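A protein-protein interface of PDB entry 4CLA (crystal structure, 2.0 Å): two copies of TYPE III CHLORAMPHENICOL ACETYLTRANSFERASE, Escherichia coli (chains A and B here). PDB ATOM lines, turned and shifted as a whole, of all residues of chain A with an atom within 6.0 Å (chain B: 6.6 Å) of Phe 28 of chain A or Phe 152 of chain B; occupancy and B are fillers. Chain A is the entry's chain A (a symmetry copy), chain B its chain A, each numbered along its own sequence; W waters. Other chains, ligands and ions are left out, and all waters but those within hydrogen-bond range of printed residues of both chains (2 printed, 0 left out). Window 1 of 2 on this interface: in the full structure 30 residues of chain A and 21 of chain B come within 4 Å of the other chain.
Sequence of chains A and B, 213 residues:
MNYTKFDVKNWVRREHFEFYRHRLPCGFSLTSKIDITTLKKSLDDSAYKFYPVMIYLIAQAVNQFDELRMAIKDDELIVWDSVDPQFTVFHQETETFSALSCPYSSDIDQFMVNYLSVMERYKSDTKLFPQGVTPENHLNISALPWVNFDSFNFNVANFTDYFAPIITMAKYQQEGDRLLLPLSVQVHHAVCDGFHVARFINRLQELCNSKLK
Phe 28 of chain A touches just these residues of chain B: Phe 152, Asn 153 and Phe 154.
Printed residues of chain A within 4 Å of Phe 152 of chain B: Phe 28, Ser 29 and Leu 30.
Printed residues of chain A within 4 Å of Asp 150 of chain B: Thr 31.
Of the printed residues of chain B, Gln 186 of chain A touches Asn 155.
Of the printed residues of chain A, Phe 149 of chain B touches Thr 31 (3.4 Å).
Of the printed residues of chain A, Ser 151 of chain B touches Leu 30 (3.3 Å) and Thr 31 (3.2 Å).
Printed residues of chain B within 4 Å of Cys 26 of chain A: Asn 155.
Thr 31 of chain B touches none of the printed residues of chain A.
Val 187 of chain A touches none of the printed residues of chain B.
Water W1 bridges OG of Ser 151 of chain B and OG of Ser 29 of chain A.
Water W2 lies within hydrogen-bond range of OD1 of Asn 155 of chain B (3.0 Å), N of Phe 28 of chain A (3.2 Å), NE2 of Gln 186 of chain A (3.3 Å) and O of Val 187 of chain A (3.4 Å).
NE2 of Gln 186 of chain B is in hydrogen-bond range of O of Phe 154 of chain B (2.9 Å).
OG1 of Thr 31 of chain B lies within hydrogen-bond range of N of Phe 152 of chain B.
The side-chain amide nitrogen (ND2) of Asn 155 of chain B lies within hydrogen-bond range of the side-chain amide oxygen (OD1) of Asn 153 of chain B (2.9 Å).
ND1 of His 188 of chain A lies within hydrogen-bond range of O of Cys 26 of chain A (3.5 Å).
The backbone carbonyl oxygen (O) of Leu 30 of chain A sits at hydrogen-bond distance from the backbone NH (N) of Val 185 of chain A.
The backbone carbonyl oxygen (O) of Phe 152 of chain B is in hydrogen-bond range of the side-chain hydroxyl (OG) of Ser 184 of chain B (3.0 Å).
The side-chain amide oxygen of Asn 153 of chain A sits at hydrogen-bond distance from the side-chain amide nitrogen of Asn 155 of chain B (3.1 Å).
O of Asn 153 of chain B sits at hydrogen-bond distance from N of Ser 29 of chain A, at 2.9 Å.
The side-chain amide oxygen of Asn 153 of chain B sits close to the side-chain amide oxygen of Asn 153 of chain A (3.4 Å).
NE2 of Gln 186 of chain A lies within hydrogen-bond range of OD1 of Asn 155 of chain B, at 3.4 Å.
N of Asn 155 of chain B lies within hydrogen-bond range of O of Gly 27 of chain A.
The backbone carbonyl oxygen (O) of Thr 31 of chain A sits at hydrogen-bond distance from the backbone NH (N) of Asp 150 of chain B.
OG1 of Thr 31 of chain A sits at hydrogen-bond distance from OG of Ser 151 of chain B.
Ser 29 of chain A touches Asn 153 of chain B, but with the chains exchanged Asn 153 of chain A does not touch Ser 29 of chain B (7.0 Å).
Asn 153 of chain A touches its own counterpart, Asn 153 of chain B.
Positions printed for both chains: 29, 30, 31, 153, 185 and 186.
Of the 18 pairs that touch across the chains among the printed residues, 1 has its exchanged pair printed and touching as well.
Hydrophobic or aromatic side chains of chain A within 4 Å of the printed part of chain B: Phe 28 and Leu 30.
Of the 16 printed residues of chain B, 8 touch a printed residue of chain A.
Hydrophobic or aromatic side chains of chain B within 4 Å of the printed part of chain A: Leu 144, Phe 149, Phe 152 and Phe 154.
Among the printed residues, 18 pairs touch across the chains.
Among the printed residues, merely in contact across the chains: Phe 28 of chain A with Asn 153 of chain B (3.2 Å), Cys 26 of chain A with Asn 155 of chain B (3.2 Å), Leu 30 of chain A with Ser 151 of chain B (3.3 Å), Ser 29 of chain A with Phe 152 of chain B (3.3 Å), Thr 31 of chain A with Phe 149 of chain B (3.4 Å), Gly 27 of chain A with Phe 154 of chain B (3.5 Å), Phe 28 of chain A with Phe 152 of chain B (3.6 Å), Gly 194 of chain A with Leu 144 of chain B (3.8 Å), Leu 30 of chain A with Leu 144 of chain B (3.9 Å), Leu 30 of chain A with Phe 152 of chain B (3.9 Å) and Phe 28 of chain A with Phe 154 of chain B (3.97 Å).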
ATOM      1  N   CYS A  26     -30.600  -7.344  33.804  1.00  0.00           N
ATOM      2  CA  CYS A  26     -30.020  -8.291  32.900  1.00  0.00           C
ATOM      3  C   CYS A  26     -28.564  -8.633  33.269  1.00  0.00           C
ATOM      4  O   CYS A  26     -27.922  -7.918  34.035  1.00  0.00           O
ATOM      5  CB  CYS A  26     -30.102  -7.800  31.500  1.00  0.00           C
ATOM      6  SG  CYS A  26     -28.892  -6.713  30.825  1.00  0.00           S
ATOM      7  N   GLY A  27     -28.229  -9.776  32.733  1.00  0.00           N
ATOM      8  CA  GLY A  27     -26.837 -10.290  32.903  1.00  0.00           C
ATOM      9  C   GLY A  27     -26.418 -10.757  31.470  1.00  0.00           C
ATOM     10  O   GLY A  27     -27.181 -10.711  30.487  1.00  0.00           O
ATOM     11  N   PHE A  28     -25.191 -11.247  31.353  1.00  0.00           N
ATOM     12  CA  PHE A  28     -24.799 -11.760  30.036  1.00  0.00           C
ATOM     13  C   PHE A  28     -23.804 -12.898  30.336  1.00  0.00           C
ATOM     14  O   PHE A  28     -23.222 -12.878  31.410  1.00  0.00           O
ATOM     15  CB  PHE A  28     -24.231 -10.664  29.120  1.00  0.00           C
ATOM     16  CG  PHE A  28     -23.028  -9.887  29.695  1.00  0.00           C
ATOM     17  CD1 PHE A  28     -21.753 -10.313  29.397  1.00  0.00           C
ATOM     18  CD2 PHE A  28     -23.202  -8.717  30.422  1.00  0.00           C
ATOM     19  CE1 PHE A  28     -20.614  -9.670  29.888  1.00  0.00           C
ATOM     20  CE2 PHE A  28     -22.127  -8.003  30.899  1.00  0.00           C
ATOM     21  CZ  PHE A  28     -20.819  -8.463  30.610  1.00  0.00           C
ATOM     22  N   SER A  29     -23.602 -13.699  29.311  1.00  0.00           N
ATOM     23  CA  SER A  29     -22.558 -14.723  29.393  1.00  0.00           C
ATOM     24  C   SER A  29     -21.732 -14.585  28.084  1.00  0.00           C
ATOM     25  O   SER A  29     -22.228 -14.087  27.067  1.00  0.00           O
ATOM     26  CB  SER A  29     -23.056 -16.150  29.541  1.00  0.00           C
ATOM     27  OG  SER A  29     -23.823 -16.462  28.341  1.00  0.00           O
ATOM     28  N   LEU A  30     -20.463 -14.974  28.183  1.00  0.00           N
ATOM     29  CA  LEU A  30     -19.581 -15.044  27.017  1.00  0.00           C
ATOM     30  C   LEU A  30     -18.667 -16.260  27.205  1.00  0.00           C
ATOM     31  O   LEU A  30     -18.266 -16.535  28.343  1.00  0.00           O
ATOM     32  CB  LEU A  30     -18.861 -13.734  26.731  1.00  0.00           C
ATOM     33  CG  LEU A  30     -17.667 -13.190  27.413  1.00  0.00           C
ATOM     34  CD1 LEU A  30     -16.352 -13.914  27.017  1.00  0.00           C
ATOM     35  CD2 LEU A  30     -17.383 -11.788  26.868  1.00  0.00           C
ATOM     36  N   THR A  31     -18.273 -16.886  26.087  1.00  0.00           N
ATOM     37  CA  THR A  31     -17.352 -18.007  26.193  1.00  0.00           C
ATOM     38  C   THR A  31     -16.155 -17.640  25.307  1.00  0.00           C
ATOM     39  O   THR A  31     -16.345 -17.221  24.142  1.00  0.00           O
ATOM     40  CB  THR A  31     -17.931 -19.359  25.679  1.00  0.00           C
ATOM     41  OG1 THR A  31     -19.213 -19.446  26.326  1.00  0.00           O
ATOM     42  CG2 THR A  31     -16.984 -20.563  25.823  1.00  0.00           C
ATOM     43  N   ASN A 153     -24.388 -21.504  28.495  1.00  0.00           N
ATOM     44  CA  ASN A 153     -25.103 -20.347  29.119  1.00  0.00           C
ATOM     45  C   ASN A 153     -26.036 -20.980  30.163  1.00  0.00           C
ATOM     46  O   ASN A 153     -26.682 -21.973  29.756  1.00  0.00           O
ATOM     47  CB  ASN A 153     -25.929 -19.609  28.023  1.00  0.00           C
ATOM     48  CG  ASN A 153     -26.759 -18.487  28.579  1.00  0.00           C
ATOM     49  OD1 ASN A 153     -28.019 -18.525  28.714  1.00  0.00           O
ATOM     50  ND2 ASN A 153     -26.123 -17.431  29.066  1.00  0.00           N
ATOM     51  N   VAL A 185     -18.016 -17.227  31.108  1.00  0.00           N
ATOM     52  CA  VAL A 185     -18.178 -16.326  32.291  1.00  0.00           C
ATOM     53  C   VAL A 185     -19.609 -15.720  32.210  1.00  0.00           C
ATOM     54  O   VAL A 185     -19.918 -15.180  31.144  1.00  0.00           O
ATOM     55  CB  VAL A 185     -17.138 -15.156  32.260  1.00  0.00           C
ATOM     56  CG1 VAL A 185     -17.239 -14.327  33.525  1.00  0.00           C
ATOM     57  CG2 VAL A 185     -15.746 -15.726  32.082  1.00  0.00           C
ATOM     58  N   GLN A 186     -20.361 -15.760  33.283  1.00  0.00           N
ATOM     59  CA  GLN A 186     -21.704 -15.236  33.297  1.00  0.00           C
ATOM     60  C   GLN A 186     -21.805 -14.276  34.463  1.00  0.00           C
ATOM     61  O   GLN A 186     -21.427 -14.644  35.565  1.00  0.00           O
ATOM     62  CB  GLN A 186     -22.649 -16.463  33.379  1.00  0.00           C
ATOM     63  CG  GLN A 186     -24.111 -16.060  33.391  1.00  0.00           C
ATOM     64  CD  GLN A 186     -25.062 -17.123  32.856  1.00  0.00           C
ATOM     65  OE1 GLN A 186     -24.599 -18.034  32.208  1.00  0.00           O
ATOM     66  NE2 GLN A 186     -26.325 -16.961  33.220  1.00  0.00           N
ATOM     67  N   VAL A 187     -22.213 -13.016  34.215  1.00  0.00           N
ATOM     68  CA  VAL A 187     -22.244 -11.991  35.286  1.00  0.00           C
ATOM     69  C   VAL A 187     -23.552 -11.202  35.180  1.00  0.00           C
ATOM     70  O   VAL A 187     -24.249 -11.248  34.159  1.00  0.00           O
ATOM     71  CB  VAL A 187     -21.007 -11.051  35.042  1.00  0.00           C
ATOM     72  CG1 VAL A 187     -19.643 -11.763  35.129  1.00  0.00           C
ATOM     73  CG2 VAL A 187     -21.077 -10.482  33.625  1.00  0.00           C
ATOM     74  N   HIS A 188     -23.774 -10.464  36.199  1.00  0.00           N
ATOM     75  CA  HIS A 188     -24.931  -9.552  36.280  1.00  0.00           C
ATOM     76  C   HIS A 188     -24.450  -8.207  35.732  1.00  0.00           C
ATOM     77  O   HIS A 188     -23.360  -7.655  36.091  1.00  0.00           O
ATOM     78  CB  HIS A 188     -25.353  -9.489  37.794  1.00  0.00           C
ATOM     79  CG  HIS A 188     -26.722  -8.872  37.902  1.00  0.00           C
ATOM     80  ND1 HIS A 188     -27.045  -7.621  37.363  1.00  0.00           N
ATOM     81  CD2 HIS A 188     -27.816  -9.356  38.522  1.00  0.00           C
ATOM     82  CE1 HIS A 188     -28.340  -7.394  37.633  1.00  0.00           C
ATOM     83  NE2 HIS A 188     -28.839  -8.402  38.332  1.00  0.00           N
ATOM     84  N   HIS A 189     -25.190  -7.609  34.793  1.00  0.00           N
ATOM     85  CA  HIS A 189     -24.800  -6.347  34.187  1.00  0.00           C
ATOM     86  C   HIS A 189     -24.846  -5.165  35.190  1.00  0.00           C
ATOM     87  O   HIS A 189     -24.198  -4.096  34.899  1.00  0.00           O
ATOM     88  CB  HIS A 189     -25.683  -5.999  32.953  1.00  0.00           C
ATOM     89  CG  HIS A 189     -24.948  -5.240  31.879  1.00  0.00           C
ATOM     90  ND1 HIS A 189     -23.963  -4.302  32.076  1.00  0.00           N
ATOM     91  CD2 HIS A 189     -25.128  -5.346  30.520  1.00  0.00           C
ATOM     92  CE1 HIS A 189     -23.541  -3.816  30.923  1.00  0.00           C
ATOM     93  NE2 HIS A 189     -24.243  -4.420  29.973  1.00  0.00           N
ATOM     94  N   CYS A 192     -20.994  -5.455  36.289  1.00  0.00           N
ATOM     95  CA  CYS A 192     -20.009  -5.716  35.298  1.00  0.00           C
ATOM     96  C   CYS A 192     -20.490  -5.379  33.859  1.00  0.00           C
ATOM     97  O   CYS A 192     -21.631  -5.717  33.532  1.00  0.00           O
ATOM     98  CB  CYS A 192     -19.598  -7.231  35.200  1.00  0.00           C
ATOM     99  SG  CYS A 192     -18.695  -7.770  36.598  1.00  0.00           S
ATOM    100  N   ASP A 193     -19.559  -4.718  33.176  1.00  0.00           N
ATOM    101  CA  ASP A 193     -19.772  -4.349  31.784  1.00  0.00           C
ATOM    102  C   ASP A 193     -18.861  -5.368  31.024  1.00  0.00           C
ATOM    103  O   ASP A 193     -18.135  -6.126  31.670  1.00  0.00           O
ATOM    104  CB  ASP A 193     -19.405  -2.905  31.511  1.00  0.00           C
ATOM    105  CG  ASP A 193     -20.234  -1.878  32.278  1.00  0.00           C
ATOM    106  OD1 ASP A 193     -19.643  -0.808  32.587  1.00  0.00           O
ATOM    107  OD2 ASP A 193     -21.457  -2.156  32.542  1.00  0.00           O
ATOM    108  N   GLY A 194     -18.911  -5.256  29.728  1.00  0.00           N
ATOM    109  CA  GLY A 194     -18.097  -6.111  28.853  1.00  0.00           C
ATOM    110  C   GLY A 194     -16.636  -5.828  29.090  1.00  0.00           C
ATOM    111  O   GLY A 194     -15.829  -6.781  29.153  1.00  0.00           O
ATOM    112  N   VAL A 197     -15.348  -7.895  32.138  1.00  0.00           N
ATOM    113  CA  VAL A 197     -15.224  -9.323  31.846  1.00  0.00           C
ATOM    114  C   VAL A 197     -13.956  -9.571  31.014  1.00  0.00           C
ATOM    115  O   VAL A 197     -13.222 -10.577  31.219  1.00  0.00           O
ATOM    116  CB  VAL A 197     -16.545  -9.822  31.193  1.00  0.00           C
ATOM    117  CG1 VAL A 197     -16.335 -11.265  30.738  1.00  0.00           C
ATOM    118  CG2 VAL A 197     -17.684  -9.829  32.202  1.00  0.00           C
ATOM    119  N   SER B  29     -30.508 -16.264  20.639  1.00  0.00           N
ATOM    120  CA  SER B  29     -29.288 -15.577  20.211  1.00  0.00           C
ATOM    121  C   SER B  29     -28.445 -16.648  19.464  1.00  0.00           C
ATOM    122  O   SER B  29     -28.596 -17.853  19.696  1.00  0.00           O
ATOM    123  CB  SER B  29     -28.464 -14.957  21.326  1.00  0.00           C
ATOM    124  OG  SER B  29     -28.023 -16.046  22.189  1.00  0.00           O
ATOM    125  N   LEU B  30     -27.626 -16.162  18.534  1.00  0.00           N
ATOM    126  CA  LEU B  30     -26.661 -17.010  17.833  1.00  0.00           C
ATOM    127  C   LEU B  30     -25.396 -16.174  17.606  1.00  0.00           C
ATOM    128  O   LEU B  30     -25.515 -14.970  17.348  1.00  0.00           O
ATOM    129  CB  LEU B  30     -27.234 -17.664  16.583  1.00  0.00           C
ATOM    130  CG  LEU B  30     -27.435 -17.051  15.253  1.00  0.00           C
ATOM    131  CD1 LEU B  30     -26.115 -16.863  14.459  1.00  0.00           C
ATOM    132  CD2 LEU B  30     -28.157 -18.057  14.351  1.00  0.00           C
ATOM    133  N   THR B  31     -24.235 -16.843  17.598  1.00  0.00           N
ATOM    134  CA  THR B  31     -23.004 -16.118  17.323  1.00  0.00           C
ATOM    135  C   THR B  31     -22.365 -16.835  16.126  1.00  0.00           C
ATOM    136  O   THR B  31     -22.253 -18.082  16.132  1.00  0.00           O
ATOM    137  CB  THR B  31     -21.978 -16.136  18.495  1.00  0.00           C
ATOM    138  OG1 THR B  31     -22.766 -15.764  19.639  1.00  0.00           O
ATOM    139  CG2 THR B  31     -20.688 -15.338  18.236  1.00  0.00           C
ATOM    140  N   LEU B 144     -17.033  -5.252  21.939  1.00  0.00           N
ATOM    141  CA  LEU B 144     -16.146  -5.685  23.015  1.00  0.00           C
ATOM    142  C   LEU B 144     -14.796  -5.892  22.339  1.00  0.00           C
ATOM    143  O   LEU B 144     -14.489  -7.029  21.992  1.00  0.00           O
ATOM    144  CB  LEU B 144     -16.544  -6.941  23.807  1.00  0.00           C
ATOM    145  CG  LEU B 144     -17.645  -6.822  24.849  1.00  0.00           C
ATOM    146  CD1 LEU B 144     -19.005  -6.703  24.177  1.00  0.00           C
ATOM    147  CD2 LEU B 144     -17.668  -8.149  25.638  1.00  0.00           C
ATOM    148  N   PHE B 149     -14.511 -13.704  21.447  1.00  0.00           N
ATOM    149  CA  PHE B 149     -15.438 -14.645  22.117  1.00  0.00           C
ATOM    150  C   PHE B 149     -15.945 -15.538  21.010  1.00  0.00           C
ATOM    151  O   PHE B 149     -15.994 -15.099  19.823  1.00  0.00           O
ATOM    152  CB  PHE B 149     -16.547 -13.950  22.960  1.00  0.00           C
ATOM    153  CG  PHE B 149     -17.511 -13.044  22.240  1.00  0.00           C
ATOM    154  CD1 PHE B 149     -18.354 -13.436  21.198  1.00  0.00           C
ATOM    155  CD2 PHE B 149     -17.561 -11.707  22.679  1.00  0.00           C
ATOM    156  CE1 PHE B 149     -19.238 -12.511  20.603  1.00  0.00           C
ATOM    157  CE2 PHE B 149     -18.475 -10.801  22.095  1.00  0.00           C
ATOM    158  CZ  PHE B 149     -19.330 -11.195  21.060  1.00  0.00           C
ATOM    159  N   ASP B 150     -16.464 -16.672  21.312  1.00  0.00           N
ATOM    160  CA  ASP B 150     -17.137 -17.587  20.371  1.00  0.00           C
ATOM    161  C   ASP B 150     -18.673 -17.514  20.662  1.00  0.00           C
ATOM    162  O   ASP B 150     -19.359 -18.019  19.757  1.00  0.00           O
ATOM    163  CB  ASP B 150     -16.678 -19.046  20.595  1.00  0.00           C
ATOM    164  CG  ASP B 150     -15.160 -19.066  20.328  1.00  0.00           C
ATOM    165  OD1 ASP B 150     -14.876 -18.827  19.179  1.00  0.00           O
ATOM    166  OD2 ASP B 150     -14.328 -19.221  21.218  1.00  0.00           O
ATOM    167  N   SER B 151     -19.050 -16.979  21.825  1.00  0.00           N
ATOM    168  CA  SER B 151     -20.485 -16.880  22.091  1.00  0.00           C
ATOM    169  C   SER B 151     -20.750 -15.690  22.977  1.00  0.00           C
ATOM    170  O   SER B 151     -19.843 -15.306  23.737  1.00  0.00           O
ATOM    171  CB  SER B 151     -21.028 -18.192  22.733  1.00  0.00           C
ATOM    172  OG  SER B 151     -21.035 -18.086  24.081  1.00  0.00           O
ATOM    173  N   PHE B 152     -21.979 -15.162  22.862  1.00  0.00           N
ATOM    174  CA  PHE B 152     -22.342 -14.039  23.721  1.00  0.00           C
ATOM    175  C   PHE B 152     -23.868 -14.191  23.924  1.00  0.00           C
ATOM    176  O   PHE B 152     -24.499 -14.343  22.851  1.00  0.00           O
ATOM    177  CB  PHE B 152     -21.938 -12.651  23.051  1.00  0.00           C
ATOM    178  CG  PHE B 152     -22.075 -11.531  24.069  1.00  0.00           C
ATOM    179  CD1 PHE B 152     -21.079 -11.052  24.965  1.00  0.00           C
ATOM    180  CD2 PHE B 152     -23.394 -10.991  24.136  1.00  0.00           C
ATOM    181  CE1 PHE B 152     -21.353  -9.994  25.876  1.00  0.00           C
ATOM    182  CE2 PHE B 152     -23.674  -9.998  25.060  1.00  0.00           C
ATOM    183  CZ  PHE B 152     -22.667  -9.486  25.921  1.00  0.00           C
ATOM    184  N   ASN B 153     -24.421 -13.959  25.092  1.00  0.00           N
ATOM    185  CA  ASN B 153     -25.915 -14.008  25.144  1.00  0.00           C
ATOM    186  C   ASN B 153     -26.301 -12.993  26.232  1.00  0.00           C
ATOM    187  O   ASN B 153     -25.633 -13.072  27.287  1.00  0.00           O
ATOM    188  CB  ASN B 153     -26.362 -15.443  25.553  1.00  0.00           C
ATOM    189  CG  ASN B 153     -27.850 -15.560  25.726  1.00  0.00           C
ATOM    190  OD1 ASN B 153     -28.437 -15.661  26.845  1.00  0.00           O
ATOM    191  ND2 ASN B 153     -28.609 -15.435  24.646  1.00  0.00           N
ATOM    192  N   PHE B 154     -27.376 -12.245  26.049  1.00  0.00           N
ATOM    193  CA  PHE B 154     -27.910 -11.378  27.129  1.00  0.00           C
ATOM    194  C   PHE B 154     -29.003 -12.180  27.871  1.00  0.00           C
ATOM    195  O   PHE B 154     -29.890 -12.600  27.092  1.00  0.00           O
ATOM    196  CB  PHE B 154     -28.583 -10.109  26.562  1.00  0.00           C
ATOM    197  CG  PHE B 154     -27.522  -9.068  26.239  1.00  0.00           C
ATOM    198  CD1 PHE B 154     -27.140  -8.812  24.933  1.00  0.00           C
ATOM    199  CD2 PHE B 154     -26.905  -8.371  27.288  1.00  0.00           C
ATOM    200  CE1 PHE B 154     -26.142  -7.856  24.616  1.00  0.00           C
ATOM    201  CE2 PHE B 154     -25.904  -7.437  27.050  1.00  0.00           C
ATOM    202  CZ  PHE B 154     -25.513  -7.195  25.688  1.00  0.00           C
ATOM    203  N   ASN B 155     -28.996 -12.271  29.168  1.00  0.00           N
ATOM    204  CA  ASN B 155     -30.094 -12.915  29.954  1.00  0.00           C
ATOM    205  C   ASN B 155     -30.898 -11.716  30.484  1.00  0.00           C
ATOM    206  O   ASN B 155     -30.394 -11.053  31.374  1.00  0.00           O
ATOM    207  CB  ASN B 155     -29.423 -13.760  31.047  1.00  0.00           C
ATOM    208  CG  ASN B 155     -28.658 -14.913  30.415  1.00  0.00           C
ATOM    209  OD1 ASN B 155     -27.421 -15.045  30.683  1.00  0.00           O
ATOM    210  ND2 ASN B 155     -29.264 -15.789  29.623  1.00  0.00           N
ATOM    211  N   ILE B 166     -30.523  -7.047  18.673  1.00  0.00           N
ATOM    212  CA  ILE B 166     -29.390  -6.686  19.553  1.00  0.00           C
ATOM    213  C   ILE B 166     -28.155  -7.267  18.912  1.00  0.00           C
ATOM    214  O   ILE B 166     -28.159  -8.508  18.731  1.00  0.00           O
ATOM    215  CB  ILE B 166     -29.643  -7.238  20.988  1.00  0.00           C
ATOM    216  CG1 ILE B 166     -30.953  -6.588  21.559  1.00  0.00           C
ATOM    217  CG2 ILE B 166     -28.412  -6.880  21.896  1.00  0.00           C
ATOM    218  CD1 ILE B 166     -31.351  -7.452  22.883  1.00  0.00           C
ATOM    219  N   THR B 168     -23.868  -7.769  18.845  1.00  0.00           N
ATOM    220  CA  THR B 168     -22.667  -7.527  19.651  1.00  0.00           C
ATOM    221  C   THR B 168     -21.482  -8.099  18.867  1.00  0.00           C
ATOM    222  O   THR B 168     -21.595  -9.246  18.420  1.00  0.00           O
ATOM    223  CB  THR B 168     -22.764  -8.236  21.039  1.00  0.00           C
ATOM    224  OG1 THR B 168     -24.041  -7.777  21.641  1.00  0.00           O
ATOM    225  CG2 THR B 168     -21.576  -7.832  21.907  1.00  0.00           C
ATOM    226  N   SER B 184     -22.678 -11.647  17.404  1.00  0.00           N
ATOM    227  CA  SER B 184     -23.806 -12.268  18.089  1.00  0.00           C
ATOM    228  C   SER B 184     -25.040 -11.472  17.746  1.00  0.00           C
ATOM    229  O   SER B 184     -24.993 -10.192  17.707  1.00  0.00           O
ATOM    230  CB  SER B 184     -23.479 -12.312  19.617  1.00  0.00           C
ATOM    231  OG  SER B 184     -24.643 -12.901  20.225  1.00  0.00           O
ATOM    232  N   VAL B 185     -26.104 -12.169  17.366  1.00  0.00           N
ATOM    233  CA  VAL B 185     -27.406 -11.511  17.037  1.00  0.00           C
ATOM    234  C   VAL B 185     -28.472 -12.098  18.006  1.00  0.00           C
ATOM    235  O   VAL B 185     -28.552 -13.330  18.055  1.00  0.00           O
ATOM    236  CB  VAL B 185     -27.843 -11.819  15.566  1.00  0.00           C
ATOM    237  CG1 VAL B 185     -29.098 -11.046  15.216  1.00  0.00           C
ATOM    238  CG2 VAL B 185     -26.705 -11.484  14.623  1.00  0.00           C
ATOM    239  N   GLN B 186     -29.254 -11.265  18.648  1.00  0.00           N
ATOM    240  CA  GLN B 186     -30.260 -11.720  19.576  1.00  0.00           C
ATOM    241  C   GLN B 186     -31.573 -11.088  19.166  1.00  0.00           C
ATOM    242  O   GLN B 186     -31.614  -9.881  18.973  1.00  0.00           O
ATOM    243  CB  GLN B 186     -29.760 -11.323  20.989  1.00  0.00           C
ATOM    244  CG  GLN B 186     -30.723 -11.751  22.079  1.00  0.00           C
ATOM    245  CD  GLN B 186     -30.076 -11.976  23.441  1.00  0.00           C
ATOM    246  OE1 GLN B 186     -28.874 -12.095  23.492  1.00  0.00           O
ATOM    247  NE2 GLN B 186     -30.923 -11.953  24.459  1.00  0.00           N
HETATM  248  O   HOH W   1     -22.819 -17.384  25.952  1.00  0.00           O
HETATM  249  O   HOH W   2     -26.403 -13.622  33.130  1.00  0.00           O
